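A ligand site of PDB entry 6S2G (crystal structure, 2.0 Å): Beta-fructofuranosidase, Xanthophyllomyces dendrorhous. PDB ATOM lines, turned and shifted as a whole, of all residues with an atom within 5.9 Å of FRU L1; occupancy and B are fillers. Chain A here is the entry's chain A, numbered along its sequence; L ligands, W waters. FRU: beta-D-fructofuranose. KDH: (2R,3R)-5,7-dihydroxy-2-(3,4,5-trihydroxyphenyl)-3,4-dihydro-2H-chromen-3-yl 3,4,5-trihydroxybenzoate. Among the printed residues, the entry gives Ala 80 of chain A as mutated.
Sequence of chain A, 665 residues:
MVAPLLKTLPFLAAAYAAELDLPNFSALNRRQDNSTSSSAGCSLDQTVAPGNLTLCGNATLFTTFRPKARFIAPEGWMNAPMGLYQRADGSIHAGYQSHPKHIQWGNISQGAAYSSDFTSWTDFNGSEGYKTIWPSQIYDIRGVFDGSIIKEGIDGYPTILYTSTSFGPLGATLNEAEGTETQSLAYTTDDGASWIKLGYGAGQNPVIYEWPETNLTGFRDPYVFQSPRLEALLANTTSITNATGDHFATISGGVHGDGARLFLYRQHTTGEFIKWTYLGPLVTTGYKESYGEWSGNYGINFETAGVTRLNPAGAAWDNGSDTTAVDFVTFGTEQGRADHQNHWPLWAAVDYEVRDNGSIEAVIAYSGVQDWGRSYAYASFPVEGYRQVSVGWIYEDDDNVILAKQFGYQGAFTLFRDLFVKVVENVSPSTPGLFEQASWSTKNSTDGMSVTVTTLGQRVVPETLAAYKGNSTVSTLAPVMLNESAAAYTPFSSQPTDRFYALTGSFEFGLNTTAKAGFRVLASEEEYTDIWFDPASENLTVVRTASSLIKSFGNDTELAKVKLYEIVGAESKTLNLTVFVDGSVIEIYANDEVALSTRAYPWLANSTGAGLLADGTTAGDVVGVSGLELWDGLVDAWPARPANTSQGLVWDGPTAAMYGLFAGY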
ATOM      1  N   ASN A  79      -5.753 -16.519  16.298  1.00  0.00           N
ATOM      2  CA  ASN A  79      -5.979 -17.101  17.602  1.00  0.00           C
ATOM      3  C   ASN A  79      -5.607 -16.128  18.748  1.00  0.00           C
ATOM      4  O   ASN A  79      -6.212 -15.053  18.820  1.00  0.00           O
ATOM      5  CB  ASN A  79      -5.522 -18.594  17.729  1.00  0.00           C
ATOM      6  CG  ASN A  79      -4.018 -18.825  17.509  1.00  0.00           C
ATOM      7  OD1 ASN A  79      -3.494 -18.713  16.393  1.00  0.00           O
ATOM      8  ND2 ASN A  79      -3.331 -19.253  18.566  1.00  0.00           N
ATOM      9  N   ALA A  80      -4.653 -16.475  19.601  1.00  0.00           N
ATOM     10  CA  ALA A  80      -4.449 -15.793  20.884  1.00  0.00           C
ATOM     11  C   ALA A  80      -4.056 -14.319  20.724  1.00  0.00           C
ATOM     12  O   ALA A  80      -3.228 -13.998  19.891  1.00  0.00           O
ATOM     13  CB  ALA A  80      -3.382 -16.505  21.674  1.00  0.00           C
ATOM     14  N   GLN A  97      -2.066 -13.741  17.288  1.00  0.00           N
ATOM     15  CA  GLN A  97      -1.563 -14.847  16.491  1.00  0.00           C
ATOM     16  C   GLN A  97      -2.380 -14.901  15.187  1.00  0.00           C
ATOM     17  O   GLN A  97      -3.612 -14.904  15.233  1.00  0.00           O
ATOM     18  CB  GLN A  97      -1.744 -16.154  17.271  1.00  0.00           C
ATOM     19  CG  GLN A  97      -0.855 -16.272  18.497  1.00  0.00           C
ATOM     20  CD  GLN A  97       0.567 -16.634  18.153  1.00  0.00           C
ATOM     21  OE1 GLN A  97       0.918 -17.811  18.047  1.00  0.00           O
ATOM     22  NE2 GLN A  97       1.424 -15.620  17.981  1.00  0.00           N
ATOM     23  N   TRP A 105      -4.316 -22.851  11.404  1.00  0.00           N
ATOM     24  CA  TRP A 105      -3.105 -22.338  12.037  1.00  0.00           C
ATOM     25  C   TRP A 105      -1.835 -22.682  11.233  1.00  0.00           C
ATOM     26  O   TRP A 105      -1.780 -23.715  10.558  1.00  0.00           O
ATOM     27  CB  TRP A 105      -3.037 -22.958  13.433  1.00  0.00           C
ATOM     28  CG  TRP A 105      -1.898 -22.563  14.360  1.00  0.00           C
ATOM     29  CD1 TRP A 105      -1.940 -21.641  15.357  1.00  0.00           C
ATOM     30  CD2 TRP A 105      -0.608 -23.176  14.422  1.00  0.00           C
ATOM     31  NE1 TRP A 105      -0.733 -21.615  16.035  1.00  0.00           N
ATOM     32  CE2 TRP A 105       0.097 -22.557  15.485  1.00  0.00           C
ATOM     33  CE3 TRP A 105       0.043 -24.184  13.681  1.00  0.00           C
ATOM     34  CZ2 TRP A 105       1.396 -22.908  15.822  1.00  0.00           C
ATOM     35  CZ3 TRP A 105       1.334 -24.534  14.025  1.00  0.00           C
ATOM     36  CH2 TRP A 105       2.004 -23.893  15.087  1.00  0.00           C
ATOM     37  N   ILE A 108       2.854 -19.031  12.208  1.00  0.00           N
ATOM     38  CA  ILE A 108       2.079 -18.134  13.062  1.00  0.00           C
ATOM     39  C   ILE A 108       2.892 -16.843  13.315  1.00  0.00           C
ATOM     40  O   ILE A 108       4.110 -16.892  13.544  1.00  0.00           O
ATOM     41  CB  ILE A 108       1.536 -18.833  14.314  1.00  0.00           C
ATOM     42  CG1 ILE A 108       0.254 -18.146  14.799  1.00  0.00           C
ATOM     43  CG2 ILE A 108       2.605 -18.929  15.411  1.00  0.00           C
ATOM     44  CD1 ILE A 108      -0.962 -18.356  13.895  1.00  0.00           C
ATOM     45  N   PHE A 145       5.218 -17.409  18.402  1.00  0.00           N
ATOM     46  CA  PHE A 145       4.140 -17.731  19.326  1.00  0.00           C
ATOM     47  C   PHE A 145       3.890 -16.521  20.230  1.00  0.00           C
ATOM     48  O   PHE A 145       4.445 -15.435  20.007  1.00  0.00           O
ATOM     49  CB  PHE A 145       4.510 -18.985  20.162  1.00  0.00           C
ATOM     50  CG  PHE A 145       4.273 -20.317  19.491  1.00  0.00           C
ATOM     51  CD1 PHE A 145       4.349 -20.479  18.107  1.00  0.00           C
ATOM     52  CD2 PHE A 145       4.051 -21.445  20.274  1.00  0.00           C
ATOM     53  CE1 PHE A 145       4.181 -21.720  17.529  1.00  0.00           C
ATOM     54  CE2 PHE A 145       3.855 -22.686  19.695  1.00  0.00           C
ATOM     55  CZ  PHE A 145       3.930 -22.825  18.319  1.00  0.00           C
ATOM     56  N   ASP A 146       3.009 -16.690  21.215  1.00  0.00           N
ATOM     57  CA  ASP A 146       2.609 -15.620  22.136  1.00  0.00           C
ATOM     58  C   ASP A 146       3.819 -14.933  22.790  1.00  0.00           C
ATOM     59  O   ASP A 146       4.857 -15.580  23.041  1.00  0.00           O
ATOM     60  CB  ASP A 146       1.716 -16.240  23.221  1.00  0.00           C
ATOM     61  CG  ASP A 146       1.006 -15.219  24.105  1.00  0.00           C
ATOM     62  OD1 ASP A 146       0.877 -14.006  23.791  1.00  0.00           O
ATOM     63  OD2 ASP A 146       0.546 -15.705  25.168  1.00  0.00           O
ATOM     64  N   THR A 163       7.724 -16.387  22.497  1.00  0.00           N
ATOM     65  CA  THR A 163       8.199 -17.738  22.233  1.00  0.00           C
ATOM     66  C   THR A 163       8.553 -17.890  20.757  1.00  0.00           C
ATOM     67  O   THR A 163       7.684 -17.854  19.883  1.00  0.00           O
ATOM     68  CB  THR A 163       7.186 -18.794  22.673  1.00  0.00           C
ATOM     69  OG1 THR A 163       6.968 -18.666  24.078  1.00  0.00           O
ATOM     70  CG2 THR A 163       7.662 -20.190  22.334  1.00  0.00           C
ATOM     71  N   ARG A 220       6.478 -22.077  26.995  1.00  0.00           N
ATOM     72  CA  ARG A 220       6.086 -20.933  26.171  1.00  0.00           C
ATOM     73  C   ARG A 220       5.259 -19.893  26.876  1.00  0.00           C
ATOM     74  O   ARG A 220       4.869 -20.053  28.048  1.00  0.00           O
ATOM     75  CB  ARG A 220       5.308 -21.448  24.934  1.00  0.00           C
ATOM     76  CG  ARG A 220       4.073 -22.285  25.228  1.00  0.00           C
ATOM     77  CD  ARG A 220       3.269 -22.552  23.945  1.00  0.00           C
ATOM     78  NE  ARG A 220       2.242 -23.585  24.118  1.00  0.00           N
ATOM     79  CZ  ARG A 220       2.489 -24.905  24.187  1.00  0.00           C
ATOM     80  NH1 ARG A 220       3.721 -25.389  24.053  1.00  0.00           N
ATOM     81  NH2 ARG A 220       1.490 -25.755  24.379  1.00  0.00           N
ATOM     82  N   ASP A 221       4.992 -18.819  26.135  1.00  0.00           N
ATOM     83  CA  ASP A 221       4.082 -17.752  26.512  1.00  0.00           C
ATOM     84  C   ASP A 221       4.644 -16.924  27.670  1.00  0.00           C
ATOM     85  O   ASP A 221       4.011 -16.778  28.705  1.00  0.00           O
ATOM     86  CB  ASP A 221       2.679 -18.301  26.817  1.00  0.00           C
ATOM     87  CG  ASP A 221       2.130 -19.163  25.685  1.00  0.00           C
ATOM     88  OD1 ASP A 221       2.640 -19.058  24.541  1.00  0.00           O
ATOM     89  OD2 ASP A 221       1.201 -19.950  25.948  1.00  0.00           O
ATOM     90  N   PHE A 302       0.013 -25.886  31.152  1.00  0.00           N
ATOM     91  CA  PHE A 302      -0.496 -24.521  31.115  1.00  0.00           C
ATOM     92  C   PHE A 302      -0.100 -23.813  29.820  1.00  0.00           C
ATOM     93  O   PHE A 302       0.973 -24.057  29.269  1.00  0.00           O
ATOM     94  CB  PHE A 302       0.066 -23.660  32.277  1.00  0.00           C
ATOM     95  CG  PHE A 302      -0.458 -24.018  33.654  1.00  0.00           C
ATOM     96  CD1 PHE A 302      -1.718 -24.573  33.875  1.00  0.00           C
ATOM     97  CD2 PHE A 302       0.336 -23.729  34.767  1.00  0.00           C
ATOM     98  CE1 PHE A 302      -2.147 -24.854  35.164  1.00  0.00           C
ATOM     99  CE2 PHE A 302      -0.107 -24.001  36.053  1.00  0.00           C
ATOM    100  CZ  PHE A 302      -1.352 -24.554  36.245  1.00  0.00           C
ATOM    101  N   GLU A 303      -0.977 -22.922  29.380  1.00  0.00           N
ATOM    102  CA  GLU A 303      -0.706 -21.976  28.313  1.00  0.00           C
ATOM    103  C   GLU A 303      -1.155 -20.574  28.709  1.00  0.00           C
ATOM    104  O   GLU A 303      -2.080 -20.398  29.521  1.00  0.00           O
ATOM    105  CB  GLU A 303      -1.425 -22.413  27.024  1.00  0.00           C
ATOM    106  CG  GLU A 303      -0.951 -23.745  26.481  1.00  0.00           C
ATOM    107  CD  GLU A 303      -1.635 -24.142  25.188  1.00  0.00           C
ATOM    108  OE1 GLU A 303      -2.881 -24.252  25.193  1.00  0.00           O
ATOM    109  OE2 GLU A 303      -0.939 -24.338  24.163  1.00  0.00           O
ATOM    110  N   THR A 304      -0.506 -19.589  28.090  1.00  0.00           N
ATOM    111  CA  THR A 304      -0.841 -18.157  28.177  1.00  0.00           C
ATOM    112  C   THR A 304      -1.087 -17.666  29.604  1.00  0.00           C
ATOM    113  O   THR A 304      -1.994 -16.871  29.843  1.00  0.00           O
ATOM    114  CB  THR A 304      -2.026 -17.747  27.248  1.00  0.00           C
ATOM    115  OG1 THR A 304      -3.287 -18.112  27.818  1.00  0.00           O
ATOM    116  CG2 THR A 304      -1.910 -18.367  25.872  1.00  0.00           C
ATOM    117  N   GLU A 334      -4.667 -27.506  29.326  1.00  0.00           N
ATOM    118  CA  GLU A 334      -4.884 -28.434  28.229  1.00  0.00           C
ATOM    119  C   GLU A 334      -5.129 -29.853  28.746  1.00  0.00           C
ATOM    120  O   GLU A 334      -4.497 -30.290  29.700  1.00  0.00           O
ATOM    121  CB  GLU A 334      -3.646 -28.509  27.349  1.00  0.00           C
ATOM    122  CG  GLU A 334      -3.126 -27.180  26.859  1.00  0.00           C
ATOM    123  CD  GLU A 334      -2.283 -27.358  25.624  1.00  0.00           C
ATOM    124  OE1 GLU A 334      -2.885 -27.443  24.534  1.00  0.00           O
ATOM    125  OE2 GLU A 334      -1.035 -27.456  25.764  1.00  0.00           O
ATOM    126  N   HIS A 343      -9.786 -27.430  26.431  1.00  0.00           N
ATOM    127  CA  HIS A 343      -9.193 -26.197  26.964  1.00  0.00           C
ATOM    128  C   HIS A 343     -10.057 -25.505  27.997  1.00  0.00           C
ATOM    129  O   HIS A 343     -11.238 -25.245  27.741  1.00  0.00           O
ATOM    130  CB  HIS A 343      -8.941 -25.221  25.821  1.00  0.00           C
ATOM    131  CG  HIS A 343      -7.713 -25.523  25.017  1.00  0.00           C
ATOM    132  ND1 HIS A 343      -7.580 -25.155  23.695  1.00  0.00           N
ATOM    133  CD2 HIS A 343      -6.571 -26.171  25.338  1.00  0.00           C
ATOM    134  CE1 HIS A 343      -6.403 -25.547  23.243  1.00  0.00           C
ATOM    135  NE2 HIS A 343      -5.772 -26.175  24.226  1.00  0.00           N
ATOM    136  N   TYR A 376     -10.563 -18.929  25.028  1.00  0.00           N
ATOM    137  CA  TYR A 376      -9.291 -19.410  25.560  1.00  0.00           C
ATOM    138  C   TYR A 376      -8.234 -18.346  25.318  1.00  0.00           C
ATOM    139  O   TYR A 376      -8.487 -17.368  24.607  1.00  0.00           O
ATOM    140  CB  TYR A 376      -8.904 -20.722  24.838  1.00  0.00           C
ATOM    141  CG  TYR A 376      -7.777 -21.517  25.463  1.00  0.00           C
ATOM    142  CD1 TYR A 376      -7.882 -22.054  26.748  1.00  0.00           C
ATOM    143  CD2 TYR A 376      -6.594 -21.767  24.760  1.00  0.00           C
ATOM    144  CE1 TYR A 376      -6.853 -22.813  27.315  1.00  0.00           C
ATOM    145  CE2 TYR A 376      -5.564 -22.497  25.319  1.00  0.00           C
ATOM    146  CZ  TYR A 376      -5.704 -23.040  26.583  1.00  0.00           C
ATOM    147  OH  TYR A 376      -4.673 -23.789  27.117  1.00  0.00           O
ATOM    148  N   ALA A 377      -7.068 -18.529  25.927  1.00  0.00           N
ATOM    149  CA  ALA A 377      -5.877 -17.727  25.657  1.00  0.00           C
ATOM    150  C   ALA A 377      -6.079 -16.267  26.079  1.00  0.00           C
ATOM    151  O   ALA A 377      -5.738 -15.343  25.354  1.00  0.00           O
ATOM    152  CB  ALA A 377      -5.466 -17.836  24.184  1.00  0.00           C
ATOM    153  N   TRP A 393      -9.581 -15.069  23.190  1.00  0.00           N
ATOM    154  CA  TRP A 393      -9.896 -15.483  21.823  1.00  0.00           C
ATOM    155  C   TRP A 393     -11.110 -16.383  21.840  1.00  0.00           C
ATOM    156  O   TRP A 393     -11.140 -17.352  22.602  1.00  0.00           O
ATOM    157  CB  TRP A 393      -8.697 -16.212  21.261  1.00  0.00           C
ATOM    158  CG  TRP A 393      -8.927 -17.176  20.115  1.00  0.00           C
ATOM    159  CD1 TRP A 393      -9.362 -16.875  18.859  1.00  0.00           C
ATOM    160  CD2 TRP A 393      -8.636 -18.569  20.119  1.00  0.00           C
ATOM    161  NE1 TRP A 393      -9.376 -18.002  18.079  1.00  0.00           N
ATOM    162  CE2 TRP A 393      -8.932 -19.065  18.828  1.00  0.00           C
ATOM    163  CE3 TRP A 393      -8.155 -19.453  21.080  1.00  0.00           C
ATOM    164  CZ2 TRP A 393      -8.752 -20.397  18.478  1.00  0.00           C
ATOM    165  CZ3 TRP A 393      -7.976 -20.791  20.747  1.00  0.00           C
ATOM    166  CH2 TRP A 393      -8.285 -21.257  19.447  1.00  0.00           C
HETATM  167  C1  FRU L   1      -2.764 -21.028  23.049  1.00  0.00           C
HETATM  168  C2  FRU L   1      -1.444 -21.151  22.289  1.00  0.00           C
HETATM  169  C3  FRU L   1      -0.258 -20.546  23.049  1.00  0.00           C
HETATM  170  C4  FRU L   1       0.733 -20.372  21.910  1.00  0.00           C
HETATM  171  C5  FRU L   1      -0.163 -20.009  20.735  1.00  0.00           C
HETATM  172  C6  FRU L   1       0.341 -20.584  19.421  1.00  0.00           C
HETATM  173  O1  FRU L   1      -3.789 -21.737  22.332  1.00  0.00           O
HETATM  174  O2  FRU L   1      -1.160 -22.531  21.993  1.00  0.00           O
HETATM  175  O3  FRU L   1       0.194 -21.404  24.091  1.00  0.00           O
HETATM  176  O4  FRU L   1       1.716 -19.343  22.099  1.00  0.00           O
HETATM  177  O5  FRU L   1      -1.467 -20.487  21.036  1.00  0.00           O
HETATM  178  O6  FRU L   1      -0.429 -20.064  18.320  1.00  0.00           O
HETATM  179  O1  KDH L   2      -0.018 -29.162  11.828  1.00  0.00           O
HETATM  180  C3  KDH L   2      -1.090 -28.874  12.625  1.00  0.00           C
HETATM  181  C6  KDH L   2      -2.390 -29.574  12.439  1.00  0.00           C
HETATM  182  O7  KDH L   2      -2.533 -30.530  11.463  1.00  0.00           O
HETATM  183  C9  KDH L   2      -3.515 -29.200  13.348  1.00  0.00           C
HETATM  184  O10 KDH L   2      -4.738 -29.793  13.242  1.00  0.00           O
HETATM  185  C12 KDH L   2      -3.315 -28.216  14.317  1.00  0.00           C
HETATM  186  C14 KDH L   2      -2.071 -27.584  14.449  1.00  0.00           C
HETATM  187  C15 KDH L   2      -1.851 -26.521  15.475  1.00  0.00           C
HETATM  188  C20 KDH L   2      -3.065 -24.914  16.819  1.00  0.00           C
HETATM  189  C21 KDH L   2      -4.113 -24.017  17.009  1.00  0.00           C
HETATM  190  C24 KDH L   2      -4.092 -23.091  18.057  1.00  0.00           C
HETATM  191  C26 KDH L   2      -3.026 -23.021  18.978  1.00  0.00           C
HETATM  192  C29 KDH L   2      -1.930 -23.890  18.847  1.00  0.00           C
HETATM  193  C31 KDH L   2      -1.907 -24.885  17.747  1.00  0.00           C
HETATM  194  C33 KDH L   2      -1.227 -27.057  16.755  1.00  0.00           C
HETATM  195  C36 KDH L   2      -2.045 -28.455  18.687  1.00  0.00           C
HETATM  196  C38 KDH L   2      -3.215 -28.506  19.637  1.00  0.00           C
HETATM  197  C39 KDH L   2      -3.238 -29.441  20.684  1.00  0.00           C
HETATM  198  C41 KDH L   2      -4.267 -27.593  19.437  1.00  0.00           C
HETATM  199  C01 KDH L   2      -0.754 -25.860  17.577  1.00  0.00           C
HETATM  200  O01 KDH L   2      -3.072 -25.827  15.781  1.00  0.00           O
HETATM  201  O02 KDH L   2      -5.146 -22.246  18.181  1.00  0.00           O
HETATM  202  O03 KDH L   2      -0.890 -23.860  19.706  1.00  0.00           O
HETATM  203  C4  KDH L   2      -0.983 -27.903  13.618  1.00  0.00           C
HETATM  204  O35 KDH L   2      -2.257 -27.847  17.380  1.00  0.00           O
HETATM  205  O37 KDH L   2      -0.944 -28.903  18.975  1.00  0.00           O
HETATM  206  C43 KDH L   2      -5.391 -27.564  20.274  1.00  0.00           C
HETATM  207  O44 KDH L   2      -6.392 -26.656  20.025  1.00  0.00           O
HETATM  208  C46 KDH L   2      -5.451 -28.537  21.399  1.00  0.00           C
HETATM  209  O47 KDH L   2      -6.505 -28.590  22.248  1.00  0.00           O
HETATM  210  C49 KDH L   2      -4.314 -29.488  21.583  1.00  0.00           C
HETATM  211  O50 KDH L   2      -4.336 -30.389  22.604  1.00  0.00           O
HETATM  212  O   HOH W   1      -3.648 -24.351  22.439  1.00  0.00           O
HETATM  213  O   HOH W   2      -4.917 -20.219  20.717  1.00  0.00           O
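The backbone NH (N) of Thr 304 sits at hydrogen-bond distance from the side-chain carboxylate (OD2) of Asp 221 (2.8 Å). N of Gln 97 sits at hydrogen-bond distance from O of Ala 80, at 2.9 Å. N of Asp 221 sits at hydrogen-bond distance from OG1 of Thr 163. OE1 of Glu 303 sits at hydrogen-bond distance from OH of Tyr 376 (2.7 Å). The guanidinium group of Arg 220 lies within salt-bridge range of the side-chain carboxylate of Glu 334 (3.3 Å). The backbone NH of Trp 393 lies within hydrogen-bond range of the backbone carbonyl oxygen of Tyr 376 (2.9 Å). The backbone carbonyl oxygen (O) of Gln 97 is in hydrogen-bond range of the backbone NH (N) of Asn 79, at 2.9 Å. The side-chain carboxylate (OE2) of Glu 303 lies within salt-bridge range of the guanidinium group (NH2) of Arg 220, at 2.8 Å.
Water W2 lies within hydrogen-bond range of O1 of FRU L1, ND2 of Asn 79 and O02 of KDH L2. Water W1 lies within hydrogen-bond range of an oxygen (O1) of FRU L1 (2.6 Å), the side-chain carboxylate of Glu 303 (2.9 Å) and a ring nitrogen (NE2) of His 343 (3.3 Å).
Phe 145 touches FRU L1. Thr 304 touches FRU L1 (CG2 to C3, 3.9 Å). Tyr 376 touches FRU L1 (CE2 to O1, 3.6 Å). Of the 18 residues printed, 10 come within 4 Å of FRU L1. Along chain A the residues within 4 Å of FRU L1 span positions 79 to 376. The nearest printed residue that does not touch FRU L1 is Ile 108 (4.1 Å).
An oxygen (O03) of KDH L2 is in hydrogen-bond range of an oxygen (O2) of FRU L1 (2.7 Å).
The guanidinium group (NE) of Arg 220 lies within hydrogen-bond range of an oxygen (O3) of FRU L1. O4 of FRU L1 is in hydrogen-bond range of N of Asp 146 (3.1 Å). O6 of FRU L1 is in hydrogen-bond range of OE1 of Gln 97 (2.6 Å). The side-chain carboxylate (OE2) of Glu 303 is in hydrogen-bond range of an oxygen (O2) of FRU L1 (2.8 Å). An oxygen (O47) of KDH L2 lies close to a ring nitrogen (NE2) of His 343. The side-chain carboxylate of Asp 221 sits at hydrogen-bond distance from an oxygen (O3) of FRU L1, at 2.6 Å. The indole nitrogen of Trp 105 lies within hydrogen-bond range of an oxygen (O6) of FRU L1, 2.8 Å away. An oxygen (O6) of FRU L1 sits at hydrogen-bond distance from the side-chain amide nitrogen (ND2) of Asn 79, 3.0 Å away.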
